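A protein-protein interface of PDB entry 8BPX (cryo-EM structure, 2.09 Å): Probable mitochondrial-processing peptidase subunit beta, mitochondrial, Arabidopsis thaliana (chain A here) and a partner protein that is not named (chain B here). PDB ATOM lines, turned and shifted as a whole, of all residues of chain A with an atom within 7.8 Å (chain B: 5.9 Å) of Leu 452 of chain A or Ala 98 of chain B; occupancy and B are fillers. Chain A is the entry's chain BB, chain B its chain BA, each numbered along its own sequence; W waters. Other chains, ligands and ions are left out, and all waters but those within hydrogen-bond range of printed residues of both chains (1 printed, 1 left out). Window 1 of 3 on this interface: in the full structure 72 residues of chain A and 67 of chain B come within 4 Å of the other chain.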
ATOM      1  N   ILE A  91       3.598  20.805  19.263  1.00  0.00           N
ATOM      2  CA  ILE A  91       2.460  21.707  19.377  1.00  0.00           C
ATOM      3  C   ILE A  91       1.130  21.005  19.152  1.00  0.00           C
ATOM      4  O   ILE A  91       0.079  21.637  19.280  1.00  0.00           O
ATOM      5  CB  ILE A  91       2.603  22.879  18.385  1.00  0.00           C
ATOM      6  CG1 ILE A  91       2.243  22.429  16.968  1.00  0.00           C
ATOM      7  CG2 ILE A  91       4.010  23.437  18.422  1.00  0.00           C
ATOM      8  CD1 ILE A  91       1.989  23.563  16.009  1.00  0.00           C
ATOM      9  N   GLN A 445      -1.689  23.280   3.629  1.00  0.00           N
ATOM     10  CA  GLN A 445      -2.950  23.999   3.737  1.00  0.00           C
ATOM     11  C   GLN A 445      -4.017  23.148   4.411  1.00  0.00           C
ATOM     12  O   GLN A 445      -4.781  23.648   5.241  1.00  0.00           O
ATOM     13  CB  GLN A 445      -3.413  24.461   2.358  1.00  0.00           C
ATOM     14  CG  GLN A 445      -2.608  25.620   1.803  1.00  0.00           C
ATOM     15  CD  GLN A 445      -3.070  26.044   0.428  1.00  0.00           C
ATOM     16  OE1 GLN A 445      -2.990  25.278  -0.530  1.00  0.00           O
ATOM     17  NE2 GLN A 445      -3.561  27.268   0.323  1.00  0.00           N
ATOM     18  N   LEU A 446      -4.081  21.856   4.075  1.00  0.00           N
ATOM     19  CA  LEU A 446      -5.094  20.988   4.665  1.00  0.00           C
ATOM     20  C   LEU A 446      -4.864  20.799   6.157  1.00  0.00           C
ATOM     21  O   LEU A 446      -5.811  20.875   6.945  1.00  0.00           O
ATOM     22  CB  LEU A 446      -5.120  19.635   3.948  1.00  0.00           C
ATOM     23  CG  LEU A 446      -6.044  18.572   4.547  1.00  0.00           C
ATOM     24  CD1 LEU A 446      -7.500  19.032   4.507  1.00  0.00           C
ATOM     25  CD2 LEU A 446      -5.878  17.236   3.841  1.00  0.00           C
ATOM     26  N   LYS A 447      -3.616  20.556   6.566  1.00  0.00           N
ATOM     27  CA  LYS A 447      -3.318  20.439   7.992  1.00  0.00           C
ATOM     28  C   LYS A 447      -3.702  21.711   8.736  1.00  0.00           C
ATOM     29  O   LYS A 447      -4.363  21.666   9.786  1.00  0.00           O
ATOM     30  CB  LYS A 447      -1.835  20.136   8.196  1.00  0.00           C
ATOM     31  CG  LYS A 447      -1.366  18.827   7.611  1.00  0.00           C
ATOM     32  CD  LYS A 447      -0.118  18.348   8.310  1.00  0.00           C
ATOM     33  CE  LYS A 447       1.110  18.567   7.447  1.00  0.00           C
ATOM     34  NZ  LYS A 447       2.242  17.692   7.854  1.00  0.00           N
ATOM     35  N   SER A 448      -3.313  22.863   8.184  1.00  0.00           N
ATOM     36  CA  SER A 448      -3.615  24.125   8.843  1.00  0.00           C
ATOM     37  C   SER A 448      -5.117  24.359   8.930  1.00  0.00           C
ATOM     38  O   SER A 448      -5.615  24.826   9.956  1.00  0.00           O
ATOM     39  CB  SER A 448      -2.926  25.276   8.113  1.00  0.00           C
ATOM     40  OG  SER A 448      -3.243  26.515   8.710  1.00  0.00           O
ATOM     41  N   SER A 449      -5.855  24.047   7.864  1.00  0.00           N
ATOM     42  CA  SER A 449      -7.293  24.290   7.874  1.00  0.00           C
ATOM     43  C   SER A 449      -8.022  23.320   8.792  1.00  0.00           C
ATOM     44  O   SER A 449      -9.050  23.678   9.375  1.00  0.00           O
ATOM     45  CB  SER A 449      -7.854  24.212   6.454  1.00  0.00           C
ATOM     46  OG  SER A 449      -7.913  22.878   5.991  1.00  0.00           O
ATOM     47  N   LEU A 450      -7.511  22.096   8.933  1.00  0.00           N
ATOM     48  CA  LEU A 450      -8.108  21.161   9.878  1.00  0.00           C
ATOM     49  C   LEU A 450      -7.868  21.598  11.314  1.00  0.00           C
ATOM     50  O   LEU A 450      -8.722  21.374  12.178  1.00  0.00           O
ATOM     51  CB  LEU A 450      -7.565  19.751   9.650  1.00  0.00           C
ATOM     52  CG  LEU A 450      -8.027  19.053   8.369  1.00  0.00           C
ATOM     53  CD1 LEU A 450      -7.283  17.746   8.151  1.00  0.00           C
ATOM     54  CD2 LEU A 450      -9.525  18.823   8.393  1.00  0.00           C
ATOM     55  N   LEU A 451      -6.755  22.293  11.568  1.00  0.00           N
ATOM     56  CA  LEU A 451      -6.401  22.674  12.965  1.00  0.00           C
ATOM     57  C   LEU A 451      -6.927  24.074  13.314  1.00  0.00           C
ATOM     58  O   LEU A 451      -7.058  24.358  14.520  1.00  0.00           O
ATOM     59  CB  LEU A 451      -4.879  22.609  13.104  1.00  0.00           C
ATOM     60  CG  LEU A 451      -4.368  21.952  14.384  1.00  0.00           C
ATOM     61  CD1 LEU A 451      -5.192  20.720  14.729  1.00  0.00           C
ATOM     62  CD2 LEU A 451      -2.899  21.592  14.250  1.00  0.00           C
ATOM     63  N   LEU A 452      -7.208  24.914  12.313  1.00  0.00           N
ATOM     64  CA  LEU A 452      -7.659  26.279  12.556  1.00  0.00           C
ATOM     65  C   LEU A 452      -9.156  26.378  12.802  1.00  0.00           C
ATOM     66  O   LEU A 452      -9.591  27.228  13.585  1.00  0.00           O
ATOM     67  CB  LEU A 452      -7.287  27.177  11.373  1.00  0.00           C
ATOM     68  CG  LEU A 452      -6.090  28.116  11.538  1.00  0.00           C
ATOM     69  CD1 LEU A 452      -4.910  27.398  12.161  1.00  0.00           C
ATOM     70  CD2 LEU A 452      -5.696  28.734  10.205  1.00  0.00           C
ATOM     71  N   HIS A 453      -9.966  25.527  12.160  1.00  0.00           N
ATOM     72  CA  HIS A 453     -11.437  25.534  12.416  1.00  0.00           C
ATOM     73  C   HIS A 453     -11.742  24.880  13.769  1.00  0.00           C
ATOM     74  O   HIS A 453     -12.924  24.887  14.169  1.00  0.00           O
ATOM     75  CB  HIS A 453     -12.200  24.861  11.262  1.00  0.00           C
ATOM     76  CG  HIS A 453     -12.364  23.384  11.407  1.00  0.00           C
ATOM     77  ND1 HIS A 453     -11.370  22.491  11.059  1.00  0.00           N
ATOM     78  CD2 HIS A 453     -13.404  22.641  11.844  1.00  0.00           C
ATOM     79  CE1 HIS A 453     -11.788  21.262  11.285  1.00  0.00           C
ATOM     80  NE2 HIS A 453     -13.032  21.327  11.769  1.00  0.00           N
ATOM     81  N   MET A 454     -10.721  24.370  14.454  1.00  0.00           N
ATOM     82  CA  MET A 454     -10.877  23.664  15.724  1.00  0.00           C
ATOM     83  C   MET A 454     -10.846  24.599  16.931  1.00  0.00           C
ATOM     84  O   MET A 454     -10.122  24.341  17.889  1.00  0.00           O
ATOM     85  CB  MET A 454      -9.770  22.627  15.835  1.00  0.00           C
ATOM     86  CG  MET A 454     -10.196  21.290  16.320  1.00  0.00           C
ATOM     87  SD  MET A 454     -11.639  20.660  15.480  1.00  0.00           S
ATOM     88  CE  MET A 454     -11.698  19.101  16.317  1.00  0.00           C
ATOM     89  N   ASP A 455     -11.632  25.671  16.932  1.00  0.00           N
ATOM     90  CA  ASP A 455     -11.655  26.574  18.078  1.00  0.00           C
ATOM     91  C   ASP A 455     -13.094  26.852  18.483  1.00  0.00           C
ATOM     92  O   ASP A 455     -13.940  27.155  17.636  1.00  0.00           O
ATOM     93  CB  ASP A 455     -10.911  27.887  17.787  1.00  0.00           C
ATOM     94  CG  ASP A 455     -11.408  28.584  16.542  1.00  0.00           C
ATOM     95  OD1 ASP A 455     -12.050  27.922  15.701  1.00  0.00           O
ATOM     96  OD2 ASP A 455     -11.148  29.797  16.403  1.00  0.00           O
ATOM     97  N   GLY A 456     -13.358  26.761  19.774  1.00  0.00           N
ATOM     98  CA  GLY A 456     -14.699  26.857  20.304  1.00  0.00           C
ATOM     99  C   GLY A 456     -15.238  25.486  20.673  1.00  0.00           C
ATOM    100  O   GLY A 456     -14.877  24.463  20.078  1.00  0.00           O
ATOM    101  N   PRO A 459     -17.457  23.442  17.567  1.00  0.00           N
ATOM    102  CA  PRO A 459     -16.741  22.645  16.557  1.00  0.00           C
ATOM    103  C   PRO A 459     -16.052  21.424  17.133  1.00  0.00           C
ATOM    104  O   PRO A 459     -16.014  20.381  16.473  1.00  0.00           O
ATOM    105  CB  PRO A 459     -15.735  23.647  15.973  1.00  0.00           C
ATOM    106  CG  PRO A 459     -16.338  24.974  16.239  1.00  0.00           C
ATOM    107  CD  PRO A 459     -16.990  24.842  17.570  1.00  0.00           C
ATOM    108  N   THR B  94      -1.431  30.377  24.467  1.00  0.00           N
ATOM    109  CA  THR B  94      -2.583  29.487  24.528  1.00  0.00           C
ATOM    110  C   THR B  94      -2.109  28.066  24.289  1.00  0.00           C
ATOM    111  O   THR B  94      -1.075  27.876  23.635  1.00  0.00           O
ATOM    112  CB  THR B  94      -3.658  29.866  23.501  1.00  0.00           C
ATOM    113  OG1 THR B  94      -4.857  29.133  23.772  1.00  0.00           O
ATOM    114  CG2 THR B  94      -3.205  29.529  22.098  1.00  0.00           C
ATOM    115  N   ASN B  96      -3.711  25.981  22.434  1.00  0.00           N
ATOM    116  CA  ASN B  96      -4.153  25.632  21.090  1.00  0.00           C
ATOM    117  C   ASN B  96      -3.002  25.790  20.096  1.00  0.00           C
ATOM    118  O   ASN B  96      -2.279  26.787  20.141  1.00  0.00           O
ATOM    119  CB  ASN B  96      -5.336  26.522  20.695  1.00  0.00           C
ATOM    120  CG  ASN B  96      -5.479  26.708  19.192  1.00  0.00           C
ATOM    121  OD1 ASN B  96      -5.336  25.772  18.408  1.00  0.00           O
ATOM    122  ND2 ASN B  96      -5.770  27.938  18.786  1.00  0.00           N
ATOM    123  N   PRO B  97      -2.812  24.833  19.184  1.00  0.00           N
ATOM    124  CA  PRO B  97      -1.722  24.950  18.199  1.00  0.00           C
ATOM    125  C   PRO B  97      -1.853  26.120  17.230  1.00  0.00           C
ATOM    126  O   PRO B  97      -0.872  26.449  16.558  1.00  0.00           O
ATOM    127  CB  PRO B  97      -1.786  23.608  17.455  1.00  0.00           C
ATOM    128  CG  PRO B  97      -3.175  23.103  17.714  1.00  0.00           C
ATOM    129  CD  PRO B  97      -3.441  23.505  19.123  1.00  0.00           C
ATOM    130  N   ALA B  98      -3.011  26.711  17.033  1.00  0.00           N
ATOM    131  CA  ALA B  98      -3.157  27.902  16.164  1.00  0.00           C
ATOM    132  C   ALA B  98      -2.770  29.251  16.795  1.00  0.00           C
ATOM    133  O   ALA B  98      -3.012  29.471  17.950  1.00  0.00           O
ATOM    134  CB  ALA B  98      -4.509  28.030  15.594  1.00  0.00           C
ATOM    135  N   ALA B  99      -2.206  30.110  15.982  1.00  0.00           N
ATOM    136  CA  ALA B  99      -1.785  31.464  16.395  1.00  0.00           C
ATOM    137  C   ALA B  99      -2.555  32.472  15.553  1.00  0.00           C
ATOM    138  O   ALA B  99      -2.894  32.156  14.452  1.00  0.00           O
ATOM    139  CB  ALA B  99      -0.291  31.637  16.294  1.00  0.00           C
ATOM    140  N   SER B 100      -2.835  33.618  16.131  1.00  0.00           N
ATOM    141  CA  SER B 100      -3.517  34.719  15.428  1.00  0.00           C
ATOM    142  C   SER B 100      -2.707  36.000  15.701  1.00  0.00           C
ATOM    143  O   SER B 100      -2.467  36.320  16.851  1.00  0.00           O
ATOM    144  CB  SER B 100      -4.974  34.787  15.831  1.00  0.00           C
ATOM    145  OG  SER B 100      -5.753  35.609  15.001  1.00  0.00           O
ATOM    146  N   GLY B 147       0.289  27.567   5.083  1.00  0.00           N
ATOM    147  CA  GLY B 147      -1.121  27.329   5.341  1.00  0.00           C
ATOM    148  C   GLY B 147      -1.818  28.463   6.055  1.00  0.00           C
ATOM    149  O   GLY B 147      -2.720  28.218   6.860  1.00  0.00           O
ATOM    150  N   GLY B 148      -1.430  29.705   5.777  1.00  0.00           N
ATOM    151  CA  GLY B 148      -1.987  30.837   6.485  1.00  0.00           C
ATOM    152  C   GLY B 148      -3.207  31.432   5.811  1.00  0.00           C
ATOM    153  O   GLY B 148      -3.524  31.143   4.662  1.00  0.00           O
ATOM    154  N   ASN B 149      -3.900  32.277   6.566  1.00  0.00           N
ATOM    155  CA  ASN B 149      -5.016  33.064   6.066  1.00  0.00           C
ATOM    156  C   ASN B 149      -4.844  34.505   6.520  1.00  0.00           C
ATOM    157  O   ASN B 149      -4.484  34.759   7.672  1.00  0.00           O
ATOM    158  CB  ASN B 149      -6.360  32.518   6.566  1.00  0.00           C
ATOM    159  CG  ASN B 149      -6.545  31.055   6.242  1.00  0.00           C
ATOM    160  OD1 ASN B 149      -6.316  30.188   7.085  1.00  0.00           O
ATOM    161  ND2 ASN B 149      -6.954  30.768   5.015  1.00  0.00           N
ATOM    162  N   ASP B 164      -3.585  34.386  10.414  1.00  0.00           N
ATOM    163  CA  ASP B 164      -3.817  33.151  11.229  1.00  0.00           C
ATOM    164  C   ASP B 164      -3.040  31.978  10.633  1.00  0.00           C
ATOM    165  O   ASP B 164      -3.091  31.792   9.469  1.00  0.00           O
ATOM    166  CB  ASP B 164      -5.296  32.772  11.293  1.00  0.00           C
ATOM    167  CG  ASP B 164      -6.281  33.800  11.816  1.00  0.00           C
ATOM    168  OD1 ASP B 164      -5.865  34.760  12.459  1.00  0.00           O
ATOM    169  OD2 ASP B 164      -7.487  33.602  11.573  1.00  0.00           O
ATOM    170  N   ALA B 165      -2.319  31.255  11.454  1.00  0.00           N
ATOM    171  CA  ALA B 165      -1.558  30.088  11.025  1.00  0.00           C
ATOM    172  C   ALA B 165      -1.195  29.264  12.254  1.00  0.00           C
ATOM    173  O   ALA B 165      -1.513  29.627  13.388  1.00  0.00           O
ATOM    174  CB  ALA B 165      -0.307  30.490  10.237  1.00  0.00           C
ATOM    175  N   LEU B 166      -0.519  28.145  12.014  1.00  0.00           N
ATOM    176  CA  LEU B 166      -0.007  27.325  13.099  1.00  0.00           C
ATOM    177  C   LEU B 166       1.095  28.064  13.853  1.00  0.00           C
ATOM    178  O   LEU B 166       1.773  28.941  13.310  1.00  0.00           O
ATOM    179  CB  LEU B 166       0.514  25.996  12.556  1.00  0.00           C
ATOM    180  CG  LEU B 166      -0.546  25.000  12.077  1.00  0.00           C
ATOM    181  CD1 LEU B 166       0.049  23.615  11.909  1.00  0.00           C
ATOM    182  CD2 LEU B 166      -1.730  24.964  13.034  1.00  0.00           C
ATOM    183  N   LYS B 167       1.273  27.690  15.123  1.00  0.00           N
ATOM    184  CA  LYS B 167       2.139  28.451  16.019  1.00  0.00           C
ATOM    185  C   LYS B 167       3.609  28.356  15.633  1.00  0.00           C
ATOM    186  O   LYS B 167       4.408  29.208  16.033  1.00  0.00           O
ATOM    187  CB  LYS B 167       1.950  27.968  17.454  1.00  0.00           C
ATOM    188  CG  LYS B 167       0.803  28.636  18.165  1.00  0.00           C
ATOM    189  CD  LYS B 167       0.463  27.963  19.490  1.00  0.00           C
ATOM    190  CE  LYS B 167       1.508  26.966  19.933  1.00  0.00           C
ATOM    191  NZ  LYS B 167       1.126  26.350  21.229  1.00  0.00           N
ATOM    192  N   SER B 263      -2.361  36.230  19.751  1.00  0.00           N
ATOM    193  CA  SER B 263      -2.868  35.137  20.624  1.00  0.00           C
ATOM    194  C   SER B 263      -2.237  33.841  20.142  1.00  0.00           C
ATOM    195  O   SER B 263      -2.444  33.508  18.985  1.00  0.00           O
ATOM    196  CB  SER B 263      -4.296  35.031  20.646  1.00  0.00           C
ATOM    197  OG  SER B 263      -4.690  34.151  21.677  1.00  0.00           O
ATOM    198  N   GLY B 264      -1.445  33.195  20.969  1.00  0.00           N
ATOM    199  CA  GLY B 264      -0.921  31.860  20.640  1.00  0.00           C
ATOM    200  C   GLY B 264       0.559  31.880  20.505  1.00  0.00           C
ATOM    201  O   GLY B 264       1.139  31.005  19.906  1.00  0.00           O
ATOM    202  N   ARG B 434     -10.284  31.997  19.037  1.00  0.00           N
ATOM    203  CA  ARG B 434      -8.947  32.640  19.191  1.00  0.00           C
ATOM    204  C   ARG B 434      -8.903  33.970  18.422  1.00  0.00           C
ATOM    205  O   ARG B 434      -8.296  34.927  18.942  1.00  0.00           O
ATOM    206  CB  ARG B 434      -7.868  31.660  18.721  1.00  0.00           C
ATOM    207  CG  ARG B 434      -6.615  32.304  18.147  1.00  0.00           C
ATOM    208  CD  ARG B 434      -5.835  31.294  17.328  1.00  0.00           C
ATOM    209  NE  ARG B 434      -6.694  30.556  16.412  1.00  0.00           N
ATOM    210  CZ  ARG B 434      -6.867  30.846  15.127  1.00  0.00           C
ATOM    211  NH1 ARG B 434      -6.227  31.866  14.583  1.00  0.00           N
ATOM    212  NH2 ARG B 434      -7.676  30.107  14.387  1.00  0.00           N
HETATM  213  O   HOH W   1      -0.446  26.953   9.247  1.00  0.00           O
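Printed residues of chain B within 4 Å of Leu 451 of chain A: Pro 97 (3.7 Å) and Leu 166 (3.8 Å). Printed residues of chain B within 4 Å of Leu 452 of chain A: Ala 98 (3.5 Å), Asn 149 (3.5 Å) and Arg 434 (3.5 Å). Of the printed residues of chain B, Asp 455 of chain A touches Arg 434. No residue of chain A comes within 4 Å of Ala 99 of chain B. Ser 100 of chain B touches none of the printed residues of chain A. The nearest residue of chain A that does not touch Ala 98 of chain B is Leu 451 of chain A (4.6 Å).
The side-chain amide oxygen of Asn 96 of chain B lies within hydrogen-bond range of the backbone NH of Ala 98 of chain B. O of Pro 97 of chain B sits at hydrogen-bond distance from N of Lys 167 of chain B, at 2.9 Å. The guanidinium group (NH1) of Arg 434 of chain B is in hydrogen-bond range of the backbone carbonyl oxygen (O) of Ala 99 of chain B. N of Asp 164 of chain B is in hydrogen-bond range of O of Asn 149 of chain B. OD1 of Asp 164 of chain B is in salt-bridge range of NH1 of Arg 434 of chain B (3.6 Å).
O of Gly 147 of chain B lies within hydrogen-bond range of OG of Ser 448 of chain A (2.6 Å).
Water W1 bridges the side-chain hydroxyl (OG) of Ser 448 of chain A and the backbone NH (N) of Leu 166 of chain B.
Of the 16 printed residues of chain B, 6 touch a printed residue of chain A. Hydrophobic or aromatic side chains of chain B within 4 Å of the printed part of chain A: Pro 97, Ala 98 and Leu 166. Among the printed residues, no Asp or Glu carboxylate lies within 4 Å of a Lys or Arg side-chain nitrogen of the other chain.
Among the printed residues, merely in contact across the chains: Ile 91 of chain A with Pro 97 of chain B (3.3 Å), Leu 451 of chain A with Pro 97 of chain B (3.7 Å), Leu 451 of chain A with Leu 166 of chain B (3.8 Å), Leu 452 of chain A with Ala 98 of chain B (3.5 Å), Leu 452 of chain A with Asn 149 of chain B (3.5 Å), Leu 452 of chain A with Arg 434 of chain B (3.5 Å) and Asp 455 of chain A with Arg 434 of chain B (3.5 Å).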
